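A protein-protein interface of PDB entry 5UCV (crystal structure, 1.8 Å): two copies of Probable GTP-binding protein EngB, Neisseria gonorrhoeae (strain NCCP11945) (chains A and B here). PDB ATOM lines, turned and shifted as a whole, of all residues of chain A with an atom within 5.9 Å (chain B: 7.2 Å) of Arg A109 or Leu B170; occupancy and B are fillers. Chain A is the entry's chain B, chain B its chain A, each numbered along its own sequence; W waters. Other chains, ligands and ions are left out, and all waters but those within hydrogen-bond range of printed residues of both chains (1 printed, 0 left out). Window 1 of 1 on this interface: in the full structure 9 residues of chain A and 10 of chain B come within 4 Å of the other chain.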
ATOM      1  N   LEU A 104     -18.617 -16.276  16.260  1.00  0.00           N
ATOM      2  CA  LEU A 104     -19.069 -17.624  15.923  1.00  0.00           C
ATOM      3  C   LEU A 104     -17.895 -18.583  15.862  1.00  0.00           C
ATOM      4  O   LEU A 104     -17.977 -19.711  16.358  1.00  0.00           O
ATOM      5  CB  LEU A 104     -19.799 -17.604  14.579  1.00  0.00           C
ATOM      6  CG  LEU A 104     -20.382 -18.935  14.100  1.00  0.00           C
ATOM      7  CD1 LEU A 104     -21.371 -19.490  15.129  1.00  0.00           C
ATOM      8  CD2 LEU A 104     -21.063 -18.713  12.742  1.00  0.00           C
ATOM      9  N   GLY A 105     -16.794 -18.152  15.243  1.00  0.00           N
ATOM     10  CA  GLY A 105     -15.597 -18.972  15.223  1.00  0.00           C
ATOM     11  C   GLY A 105     -15.110 -19.322  16.618  1.00  0.00           C
ATOM     12  O   GLY A 105     -14.751 -20.473  16.895  1.00  0.00           O
ATOM     13  N   ASP A 106     -15.109 -18.343  17.520  1.00  0.00           N
ATOM     14  CA  ASP A 106     -14.720 -18.617  18.904  1.00  0.00           C
ATOM     15  C   ASP A 106     -15.674 -19.591  19.600  1.00  0.00           C
ATOM     16  O   ASP A 106     -15.243 -20.410  20.421  1.00  0.00           O
ATOM     17  CB  ASP A 106     -14.657 -17.321  19.693  1.00  0.00           C
ATOM     18  CG  ASP A 106     -14.348 -17.565  21.143  1.00  0.00           C
ATOM     19  OD1 ASP A 106     -13.197 -17.934  21.442  1.00  0.00           O
ATOM     20  OD2 ASP A 106     -15.265 -17.422  21.972  1.00  0.00           O
ATOM     21  N   TYR A 107     -16.977 -19.474  19.335  1.00  0.00           N
ATOM     22  CA  TYR A 107     -17.936 -20.440  19.870  1.00  0.00           C
ATOM     23  C   TYR A 107     -17.619 -21.860  19.391  1.00  0.00           C
ATOM     24  O   TYR A 107     -17.581 -22.809  20.191  1.00  0.00           O
ATOM     25  CB  TYR A 107     -19.357 -20.010  19.480  1.00  0.00           C
ATOM     26  CG  TYR A 107     -20.397 -21.105  19.579  1.00  0.00           C
ATOM     27  CD1 TYR A 107     -20.666 -21.924  18.491  1.00  0.00           C
ATOM     28  CD2 TYR A 107     -21.116 -21.307  20.748  1.00  0.00           C
ATOM     29  CE1 TYR A 107     -21.609 -22.933  18.566  1.00  0.00           C
ATOM     30  CE2 TYR A 107     -22.075 -22.318  20.829  1.00  0.00           C
ATOM     31  CZ  TYR A 107     -22.312 -23.124  19.733  1.00  0.00           C
ATOM     32  OH  TYR A 107     -23.246 -24.141  19.794  1.00  0.00           O
ATOM     33  N   LEU A 108     -17.372 -22.030  18.089  1.00  0.00           N
ATOM     34  CA  LEU A 108     -16.993 -23.360  17.604  1.00  0.00           C
ATOM     35  C   LEU A 108     -15.725 -23.868  18.290  1.00  0.00           C
ATOM     36  O   LEU A 108     -15.633 -25.044  18.658  1.00  0.00           O
ATOM     37  CB  LEU A 108     -16.807 -23.333  16.088  1.00  0.00           C
ATOM     38  CG  LEU A 108     -18.103 -22.999  15.324  1.00  0.00           C
ATOM     39  CD1 LEU A 108     -17.813 -22.904  13.810  1.00  0.00           C
ATOM     40  CD2 LEU A 108     -19.160 -24.058  15.603  1.00  0.00           C
ATOM     41  N   ARG A 109     -14.731 -22.997  18.458  1.00  0.00           N
ATOM     42  CA  ARG A 109     -13.466 -23.414  19.050  1.00  0.00           C
ATOM     43  C   ARG A 109     -13.611 -23.777  20.529  1.00  0.00           C
ATOM     44  O   ARG A 109     -12.919 -24.689  21.016  1.00  0.00           O
ATOM     45  CB  ARG A 109     -12.444 -22.284  18.864  1.00  0.00           C
ATOM     46  CG  ARG A 109     -11.126 -22.424  19.592  1.00  0.00           C
ATOM     47  CD  ARG A 109     -10.280 -21.170  19.292  1.00  0.00           C
ATOM     48  NE  ARG A 109      -9.719 -21.191  17.934  1.00  0.00           N
ATOM     49  CZ  ARG A 109      -9.317 -20.111  17.256  1.00  0.00           C
ATOM     50  NH1 ARG A 109      -9.473 -18.901  17.784  1.00  0.00           N
ATOM     51  NH2 ARG A 109      -8.788 -20.243  16.033  1.00  0.00           N
ATOM     52  N   HIS A 110     -14.509 -23.101  21.254  1.00  0.00           N
ATOM     53  CA  HIS A 110     -14.445 -23.102  22.713  1.00  0.00           C
ATOM     54  C   HIS A 110     -15.684 -23.604  23.443  1.00  0.00           C
ATOM     55  O   HIS A 110     -15.596 -23.830  24.656  1.00  0.00           O
ATOM     56  CB  HIS A 110     -14.128 -21.685  23.229  1.00  0.00           C
ATOM     57  CG  HIS A 110     -12.680 -21.320  23.116  1.00  0.00           C
ATOM     58  ND1 HIS A 110     -12.247 -20.139  22.549  1.00  0.00           N
ATOM     59  CD2 HIS A 110     -11.564 -21.989  23.492  1.00  0.00           C
ATOM     60  CE1 HIS A 110     -10.926 -20.097  22.589  1.00  0.00           C
ATOM     61  NE2 HIS A 110     -10.488 -21.209  23.155  1.00  0.00           N
ATOM     62  N   ARG A 111     -16.827 -23.769  22.780  1.00  0.00           N
ATOM     63  CA  ARG A 111     -18.043 -24.173  23.485  1.00  0.00           C
ATOM     64  C   ARG A 111     -17.876 -25.605  23.988  1.00  0.00           C
ATOM     65  O   ARG A 111     -17.835 -26.544  23.191  1.00  0.00           O
ATOM     66  CB  ARG A 111     -19.256 -24.058  22.563  1.00  0.00           C
ATOM     67  CG  ARG A 111     -20.583 -24.500  23.200  1.00  0.00           C
ATOM     68  CD  ARG A 111     -21.115 -23.458  24.187  1.00  0.00           C
ATOM     69  NE  ARG A 111     -22.549 -23.662  24.381  1.00  0.00           N
ATOM     70  CZ  ARG A 111     -23.245 -23.179  25.406  1.00  0.00           C
ATOM     71  NH1 ARG A 111     -22.650 -22.451  26.350  1.00  0.00           N
ATOM     72  NH2 ARG A 111     -24.546 -23.414  25.475  1.00  0.00           N
ATOM     73  N   ARG A 133     -13.343 -21.511   6.864  1.00  0.00           N
ATOM     74  CA  ARG A 133     -12.874 -20.887   8.099  1.00  0.00           C
ATOM     75  C   ARG A 133     -13.604 -21.468   9.301  1.00  0.00           C
ATOM     76  O   ARG A 133     -12.994 -21.732  10.343  1.00  0.00           O
ATOM     77  CB  ARG A 133     -13.052 -19.368   8.052  1.00  0.00           C
ATOM     78  CG  ARG A 133     -12.131 -18.642   9.048  1.00  0.00           C
ATOM     79  CD  ARG A 133     -12.425 -17.139   9.135  1.00  0.00           C
ATOM     80  NE  ARG A 133     -12.413 -16.467   7.836  1.00  0.00           N
ATOM     81  CZ  ARG A 133     -12.529 -15.149   7.694  1.00  0.00           C
ATOM     82  NH1 ARG A 133     -12.648 -14.382   8.770  1.00  0.00           N
ATOM     83  NH2 ARG A 133     -12.526 -14.591   6.486  1.00  0.00           N
ATOM     84  N   ASP A 136     -12.215 -24.764  10.068  1.00  0.00           N
ATOM     85  CA  ASP A 136     -10.927 -24.637  10.738  1.00  0.00           C
ATOM     86  C   ASP A 136     -11.111 -24.258  12.202  1.00  0.00           C
ATOM     87  O   ASP A 136     -10.399 -24.770  13.078  1.00  0.00           O
ATOM     88  CB  ASP A 136     -10.048 -23.610  10.010  1.00  0.00           C
ATOM     89  CG  ASP A 136      -9.519 -24.131   8.681  1.00  0.00           C
ATOM     90  OD1 ASP A 136      -9.624 -25.357   8.422  1.00  0.00           O
ATOM     91  OD2 ASP A 136      -8.985 -23.306   7.897  1.00  0.00           O
ATOM     92  N   PHE A 137     -12.054 -23.351  12.491  1.00  0.00           N
ATOM     93  CA  PHE A 137     -12.304 -22.983  13.880  1.00  0.00           C
ATOM     94  C   PHE A 137     -12.703 -24.205  14.701  1.00  0.00           C
ATOM     95  O   PHE A 137     -12.299 -24.344  15.858  1.00  0.00           O
ATOM     96  CB  PHE A 137     -13.414 -21.932  13.968  1.00  0.00           C
ATOM     97  CG  PHE A 137     -12.944 -20.506  13.810  1.00  0.00           C
ATOM     98  CD1 PHE A 137     -12.053 -19.948  14.719  1.00  0.00           C
ATOM     99  CD2 PHE A 137     -13.441 -19.715  12.785  1.00  0.00           C
ATOM    100  CE1 PHE A 137     -11.651 -18.618  14.587  1.00  0.00           C
ATOM    101  CE2 PHE A 137     -13.064 -18.393  12.648  1.00  0.00           C
ATOM    102  CZ  PHE A 137     -12.151 -17.842  13.540  1.00  0.00           C
ATOM    103  N   PHE A 138     -13.507 -25.098  14.110  1.00  0.00           N
ATOM    104  CA  PHE A 138     -14.033 -26.250  14.828  1.00  0.00           C
ATOM    105  C   PHE A 138     -13.058 -27.413  14.875  1.00  0.00           C
ATOM    106  O   PHE A 138     -13.184 -28.277  15.745  1.00  0.00           O
ATOM    107  CB  PHE A 138     -15.340 -26.711  14.163  1.00  0.00           C
ATOM    108  CG  PHE A 138     -16.145 -27.670  14.993  1.00  0.00           C
ATOM    109  CD1 PHE A 138     -16.519 -27.343  16.288  1.00  0.00           C
ATOM    110  CD2 PHE A 138     -16.537 -28.895  14.472  1.00  0.00           C
ATOM    111  CE1 PHE A 138     -17.277 -28.232  17.059  1.00  0.00           C
ATOM    112  CE2 PHE A 138     -17.302 -29.778  15.231  1.00  0.00           C
ATOM    113  CZ  PHE A 138     -17.671 -29.441  16.523  1.00  0.00           C
ATOM    114  N   THR A 140     -10.002 -28.088  15.754  1.00  0.00           N
ATOM    115  CA  THR A 140      -9.188 -28.437  16.917  1.00  0.00           C
ATOM    116  C   THR A 140      -9.973 -29.155  18.017  1.00  0.00           C
ATOM    117  O   THR A 140      -9.346 -29.691  18.938  1.00  0.00           O
ATOM    118  CB  THR A 140      -8.512 -27.178  17.489  1.00  0.00           C
ATOM    119  OG1 THR A 140      -9.497 -26.173  17.743  1.00  0.00           O
ATOM    120  CG2 THR A 140      -7.502 -26.624  16.478  1.00  0.00           C
ATOM    121  N   THR A 141     -11.312 -29.170  17.959  1.00  0.00           N
ATOM    122  CA  THR A 141     -12.111 -29.901  18.946  1.00  0.00           C
ATOM    123  C   THR A 141     -12.065 -31.403  18.722  1.00  0.00           C
ATOM    124  O   THR A 141     -12.384 -32.172  19.645  1.00  0.00           O
ATOM    125  CB  THR A 141     -13.591 -29.502  18.899  1.00  0.00           C
ATOM    126  OG1 THR A 141     -14.152 -29.920  17.647  1.00  0.00           O
ATOM    127  CG2 THR A 141     -13.800 -27.984  19.099  1.00  0.00           C
ATOM    128  N   PRO B 126       0.269 -24.974  11.366  1.00  0.00           N
ATOM    129  CA  PRO B 126       0.071 -24.057  12.492  1.00  0.00           C
ATOM    130  C   PRO B 126      -1.261 -24.288  13.193  1.00  0.00           C
ATOM    131  O   PRO B 126      -2.177 -24.923  12.663  1.00  0.00           O
ATOM    132  CB  PRO B 126       0.097 -22.679  11.827  1.00  0.00           C
ATOM    133  CG  PRO B 126      -0.478 -22.941  10.501  1.00  0.00           C
ATOM    134  CD  PRO B 126       0.022 -24.296  10.076  1.00  0.00           C
ATOM    135  N   LEU B 127      -1.338 -23.750  14.414  1.00  0.00           N
ATOM    136  CA  LEU B 127      -2.579 -23.666  15.189  1.00  0.00           C
ATOM    137  C   LEU B 127      -3.208 -25.046  15.397  1.00  0.00           C
ATOM    138  O   LEU B 127      -4.366 -25.298  15.049  1.00  0.00           O
ATOM    139  CB  LEU B 127      -3.571 -22.699  14.532  1.00  0.00           C
ATOM    140  CG  LEU B 127      -3.236 -21.215  14.585  1.00  0.00           C
ATOM    141  CD1 LEU B 127      -4.376 -20.444  13.940  1.00  0.00           C
ATOM    142  CD2 LEU B 127      -3.019 -20.737  16.021  1.00  0.00           C
ATOM    143  N   ILE B 132      -3.628 -23.538  20.507  1.00  0.00           N
ATOM    144  CA  ILE B 132      -4.799 -22.826  21.012  1.00  0.00           C
ATOM    145  C   ILE B 132      -4.808 -22.849  22.531  1.00  0.00           C
ATOM    146  O   ILE B 132      -5.112 -21.844  23.189  1.00  0.00           O
ATOM    147  CB  ILE B 132      -6.086 -23.447  20.434  1.00  0.00           C
ATOM    148  CG1 ILE B 132      -6.110 -23.297  18.902  1.00  0.00           C
ATOM    149  CG2 ILE B 132      -7.329 -22.815  21.076  1.00  0.00           C
ATOM    150  CD1 ILE B 132      -6.040 -21.879  18.459  1.00  0.00           C
ATOM    151  N   LEU B 135      -2.477 -20.213  23.879  1.00  0.00           N
ATOM    152  CA  LEU B 135      -3.051 -18.883  23.713  1.00  0.00           C
ATOM    153  C   LEU B 135      -4.156 -18.645  24.735  1.00  0.00           C
ATOM    154  O   LEU B 135      -4.279 -17.540  25.285  1.00  0.00           O
ATOM    155  CB  LEU B 135      -3.585 -18.715  22.287  1.00  0.00           C
ATOM    156  CG  LEU B 135      -2.509 -18.632  21.203  1.00  0.00           C
ATOM    157  CD1 LEU B 135      -3.149 -18.931  19.858  1.00  0.00           C
ATOM    158  CD2 LEU B 135      -1.885 -17.240  21.188  1.00  0.00           C
ATOM    159  N   ASP B 136      -4.951 -19.683  25.028  1.00  0.00           N
ATOM    160  CA  ASP B 136      -6.022 -19.525  26.008  1.00  0.00           C
ATOM    161  C   ASP B 136      -5.463 -19.318  27.412  1.00  0.00           C
ATOM    162  O   ASP B 136      -5.988 -18.504  28.183  1.00  0.00           O
ATOM    163  CB  ASP B 136      -6.950 -20.742  25.994  1.00  0.00           C
ATOM    164  CG  ASP B 136      -7.706 -20.874  24.702  1.00  0.00           C
ATOM    165  OD1 ASP B 136      -7.829 -19.854  23.984  1.00  0.00           O
ATOM    166  OD2 ASP B 136      -8.167 -21.998  24.409  1.00  0.00           O
ATOM    167  N   LEU B 164      -0.027 -17.326   6.261  1.00  0.00           N
ATOM    168  CA  LEU B 164      -0.129 -16.061   6.987  1.00  0.00           C
ATOM    169  C   LEU B 164      -1.573 -15.603   7.086  1.00  0.00           C
ATOM    170  O   LEU B 164      -2.055 -15.247   8.170  1.00  0.00           O
ATOM    171  CB  LEU B 164       0.689 -14.970   6.293  1.00  0.00           C
ATOM    172  CG  LEU B 164       2.106 -14.616   6.708  1.00  0.00           C
ATOM    173  CD1 LEU B 164       2.579 -13.511   5.786  1.00  0.00           C
ATOM    174  CD2 LEU B 164       2.166 -14.168   8.164  1.00  0.00           C
ATOM    175  N   SER B 165      -2.278 -15.594   5.949  1.00  0.00           N
ATOM    176  CA  SER B 165      -3.662 -15.133   5.927  1.00  0.00           C
ATOM    177  C   SER B 165      -4.550 -15.999   6.813  1.00  0.00           C
ATOM    178  O   SER B 165      -5.358 -15.486   7.599  1.00  0.00           O
ATOM    179  CB  SER B 165      -4.178 -15.135   4.486  1.00  0.00           C
ATOM    180  OG  SER B 165      -5.519 -14.698   4.428  1.00  0.00           O
ATOM    181  N   GLN B 166      -4.428 -17.320   6.689  1.00  0.00           N
ATOM    182  CA  GLN B 166      -5.345 -18.182   7.430  1.00  0.00           C
ATOM    183  C   GLN B 166      -5.083 -18.113   8.930  1.00  0.00           C
ATOM    184  O   GLN B 166      -6.029 -18.069   9.720  1.00  0.00           O
ATOM    185  CB  GLN B 166      -5.266 -19.626   6.922  1.00  0.00           C
ATOM    186  CG  GLN B 166      -6.514 -20.479   7.288  1.00  0.00           C
ATOM    187  CD  GLN B 166      -7.831 -20.003   6.633  1.00  0.00           C
ATOM    188  OE1 GLN B 166      -7.836 -19.109   5.770  1.00  0.00           O
ATOM    189  NE2 GLN B 166      -8.959 -20.621   7.038  1.00  0.00           N
ATOM    190  N   VAL B 167      -3.811 -18.063   9.341  1.00  0.00           N
ATOM    191  CA  VAL B 167      -3.509 -17.942  10.769  1.00  0.00           C
ATOM    192  C   VAL B 167      -4.041 -16.623  11.320  1.00  0.00           C
ATOM    193  O   VAL B 167      -4.640 -16.580  12.401  1.00  0.00           O
ATOM    194  CB  VAL B 167      -1.993 -18.082  11.013  1.00  0.00           C
ATOM    195  CG1 VAL B 167      -1.652 -17.705  12.444  1.00  0.00           C
ATOM    196  CG2 VAL B 167      -1.536 -19.502  10.711  1.00  0.00           C
ATOM    197  N   LYS B 168      -3.832 -15.520  10.589  1.00  0.00           N
ATOM    198  CA  LYS B 168      -4.324 -14.233  11.076  1.00  0.00           C
ATOM    199  C   LYS B 168      -5.846 -14.243  11.216  1.00  0.00           C
ATOM    200  O   LYS B 168      -6.387 -13.753  12.216  1.00  0.00           O
ATOM    201  CB  LYS B 168      -3.837 -13.099  10.152  1.00  0.00           C
ATOM    202  CG  LYS B 168      -2.333 -12.784  10.377  1.00  0.00           C
ATOM    203  CD  LYS B 168      -1.697 -11.882   9.282  1.00  0.00           C
ATOM    204  CE  LYS B 168      -2.379 -10.529   9.171  1.00  0.00           C
ATOM    205  NZ  LYS B 168      -2.098  -9.660  10.370  1.00  0.00           N
ATOM    206  N   LYS B 169      -6.555 -14.818  10.240  1.00  0.00           N
ATOM    207  CA  LYS B 169      -8.009 -14.902  10.364  1.00  0.00           C
ATOM    208  C   LYS B 169      -8.408 -15.720  11.590  1.00  0.00           C
ATOM    209  O   LYS B 169      -9.309 -15.331  12.344  1.00  0.00           O
ATOM    210  CB  LYS B 169      -8.606 -15.513   9.102  1.00  0.00           C
ATOM    211  CG  LYS B 169      -8.546 -14.605   7.883  1.00  0.00           C
ATOM    212  CD  LYS B 169      -8.845 -15.440   6.642  1.00  0.00           C
ATOM    213  CE  LYS B 169      -8.760 -14.616   5.356  1.00  0.00           C
ATOM    214  NZ  LYS B 169      -9.118 -15.459   4.169  1.00  0.00           N
ATOM    215  N   LEU B 170      -7.744 -16.851  11.810  1.00  0.00           N
ATOM    216  CA  LEU B 170      -8.159 -17.722  12.905  1.00  0.00           C
ATOM    217  C   LEU B 170      -7.788 -17.149  14.266  1.00  0.00           C
ATOM    218  O   LEU B 170      -8.352 -17.582  15.278  1.00  0.00           O
ATOM    219  CB  LEU B 170      -7.560 -19.122  12.734  1.00  0.00           C
ATOM    220  CG  LEU B 170      -8.128 -19.888  11.535  1.00  0.00           C
ATOM    221  CD1 LEU B 170      -7.277 -21.105  11.184  1.00  0.00           C
ATOM    222  CD2 LEU B 170      -9.586 -20.327  11.788  1.00  0.00           C
ATOM    223  N   LEU B 171      -6.868 -16.177  14.321  1.00  0.00           N
ATOM    224  CA  LEU B 171      -6.491 -15.570  15.594  1.00  0.00           C
ATOM    225  C   LEU B 171      -7.238 -14.280  15.895  1.00  0.00           C
ATOM    226  O   LEU B 171      -7.094 -13.747  16.998  1.00  0.00           O
ATOM    227  CB  LEU B 171      -4.983 -15.298  15.631  1.00  0.00           C
ATOM    228  CG  LEU B 171      -4.107 -16.549  15.696  1.00  0.00           C
ATOM    229  CD1 LEU B 171      -2.640 -16.181  15.787  1.00  0.00           C
ATOM    230  CD2 LEU B 171      -4.534 -17.438  16.862  1.00  0.00           C
ATOM    231  N   LYS B 172      -8.042 -13.783  14.968  1.00  0.00           N
ATOM    232  CA  LYS B 172      -8.757 -12.528  15.177  1.00  0.00           C
ATOM    233  C   LYS B 172      -9.604 -12.526  16.451  1.00  0.00           C
ATOM    234  O   LYS B 172      -9.724 -11.464  17.077  1.00  0.00           O
ATOM    235  CB  LYS B 172      -9.636 -12.194  13.961  1.00  0.00           C
ATOM    236  N   PRO B 173     -10.205 -13.645  16.889  1.00  0.00           N
ATOM    237  CA  PRO B 173     -10.979 -13.575  18.139  1.00  0.00           C
ATOM    238  C   PRO B 173     -10.160 -13.137  19.341  1.00  0.00           C
ATOM    239  O   PRO B 173     -10.718 -12.537  20.266  1.00  0.00           O
ATOM    240  CB  PRO B 173     -11.517 -15.004  18.302  1.00  0.00           C
ATOM    241  CG  PRO B 173     -11.678 -15.491  16.920  1.00  0.00           C
ATOM    242  CD  PRO B 173     -10.482 -14.912  16.171  1.00  0.00           C
ATOM    243  N   TYR B 174      -8.855 -13.417  19.361  1.00  0.00           N
ATOM    244  CA  TYR B 174      -8.031 -13.011  20.494  1.00  0.00           C
ATOM    245  C   TYR B 174      -7.749 -11.515  20.506  1.00  0.00           C
ATOM    246  O   TYR B 174      -7.274 -11.002  21.523  1.00  0.00           O
ATOM    247  CB  TYR B 174      -6.703 -13.790  20.491  1.00  0.00           C
ATOM    248  CG  TYR B 174      -6.876 -15.274  20.735  1.00  0.00           C
ATOM    249  CD1 TYR B 174      -6.967 -15.772  22.024  1.00  0.00           C
ATOM    250  CD2 TYR B 174      -6.944 -16.174  19.682  1.00  0.00           C
ATOM    251  CE1 TYR B 174      -7.132 -17.121  22.262  1.00  0.00           C
ATOM    252  CE2 TYR B 174      -7.110 -17.532  19.918  1.00  0.00           C
ATOM    253  CZ  TYR B 174      -7.203 -17.994  21.203  1.00  0.00           C
ATOM    254  OH  TYR B 174      -7.362 -19.344  21.423  1.00  0.00           O
HETATM  255  O   HOH W   1     -11.899 -14.668  11.633  1.00  0.00           O
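A ring nitrogen (NE2) of His A110 is in hydrogen-bond range of the side-chain carboxylate (OD2) of Asp B136. The side-chain amide nitrogen of Gln B166 is in hydrogen-bond range of the side-chain carboxylate of Asp A136, at 2.8 Å. O of Leu B170 sits at hydrogen-bond distance from NH2 of Arg A109 (2.8 Å).
The side-chain carboxylate of Asp B136 is in hydrogen-bond range of the side-chain hydroxyl of Tyr B174 (2.7 Å). The side-chain carboxylate (OD1) of Asp A106 sits at hydrogen-bond distance from a ring nitrogen (ND1) of His A110, at 2.6 Å.
1 position is printed for both chains. Of the 13 pairs that touch across the chains among the printed residues, none has its exchanged pair printed and touching as well.
Of the 16 printed residues of chain B, 8 touch a printed residue of chain A. Hydrophobic or aromatic side chains of chain B that line the printed part of chain A: Ile B132, Leu B170, Pro B173 and Tyr B174. Of the 14 printed residues of chain A, 6 touch a printed residue of chain B. Among the printed residues, no Asp or Glu carboxylate lies within 4 Å of a Lys or Arg side-chain nitrogen of the other chain.
Water W1 bridges O of Lys B169 (2.8 Å) and NH1 of Arg A133 (3.0 Å).
Arg A109 touches just these residues of chain B: Ile B132, Leu B170 and Tyr B174. Of the printed residues of chain B, Phe A137 touches Lys B169, Leu B170 and Pro B173. Printed residues of chain A within 4 Å of Asp B136: His A110 (2.8 Å). Ser B165 touches none of the printed residues of chain A.
NE of Arg A109 touches CD1 of Ile B132, 3.8 Å away. NH1 of Arg A109 touches CE2 of Tyr B174, at 3.5 Å. OH of Tyr B174 touches CE1 of His A110, at 3.8 Å. NH2 of Arg A133 touches CD of Lys B169, 3.8 Å away. Leu B170 touches Arg A133 (CD2 to O, 3.96 Å). CD2 of Leu B170 touches CB of Asp A136, 3.8 Å away. CZ of Phe A137 touches O of Lys B169, at 3.98 Å. Leu B170 touches Phe A137. Phe A137 touches Pro B173. O of Leu B127 touches CG2 of Thr A140 (3.7 Å).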
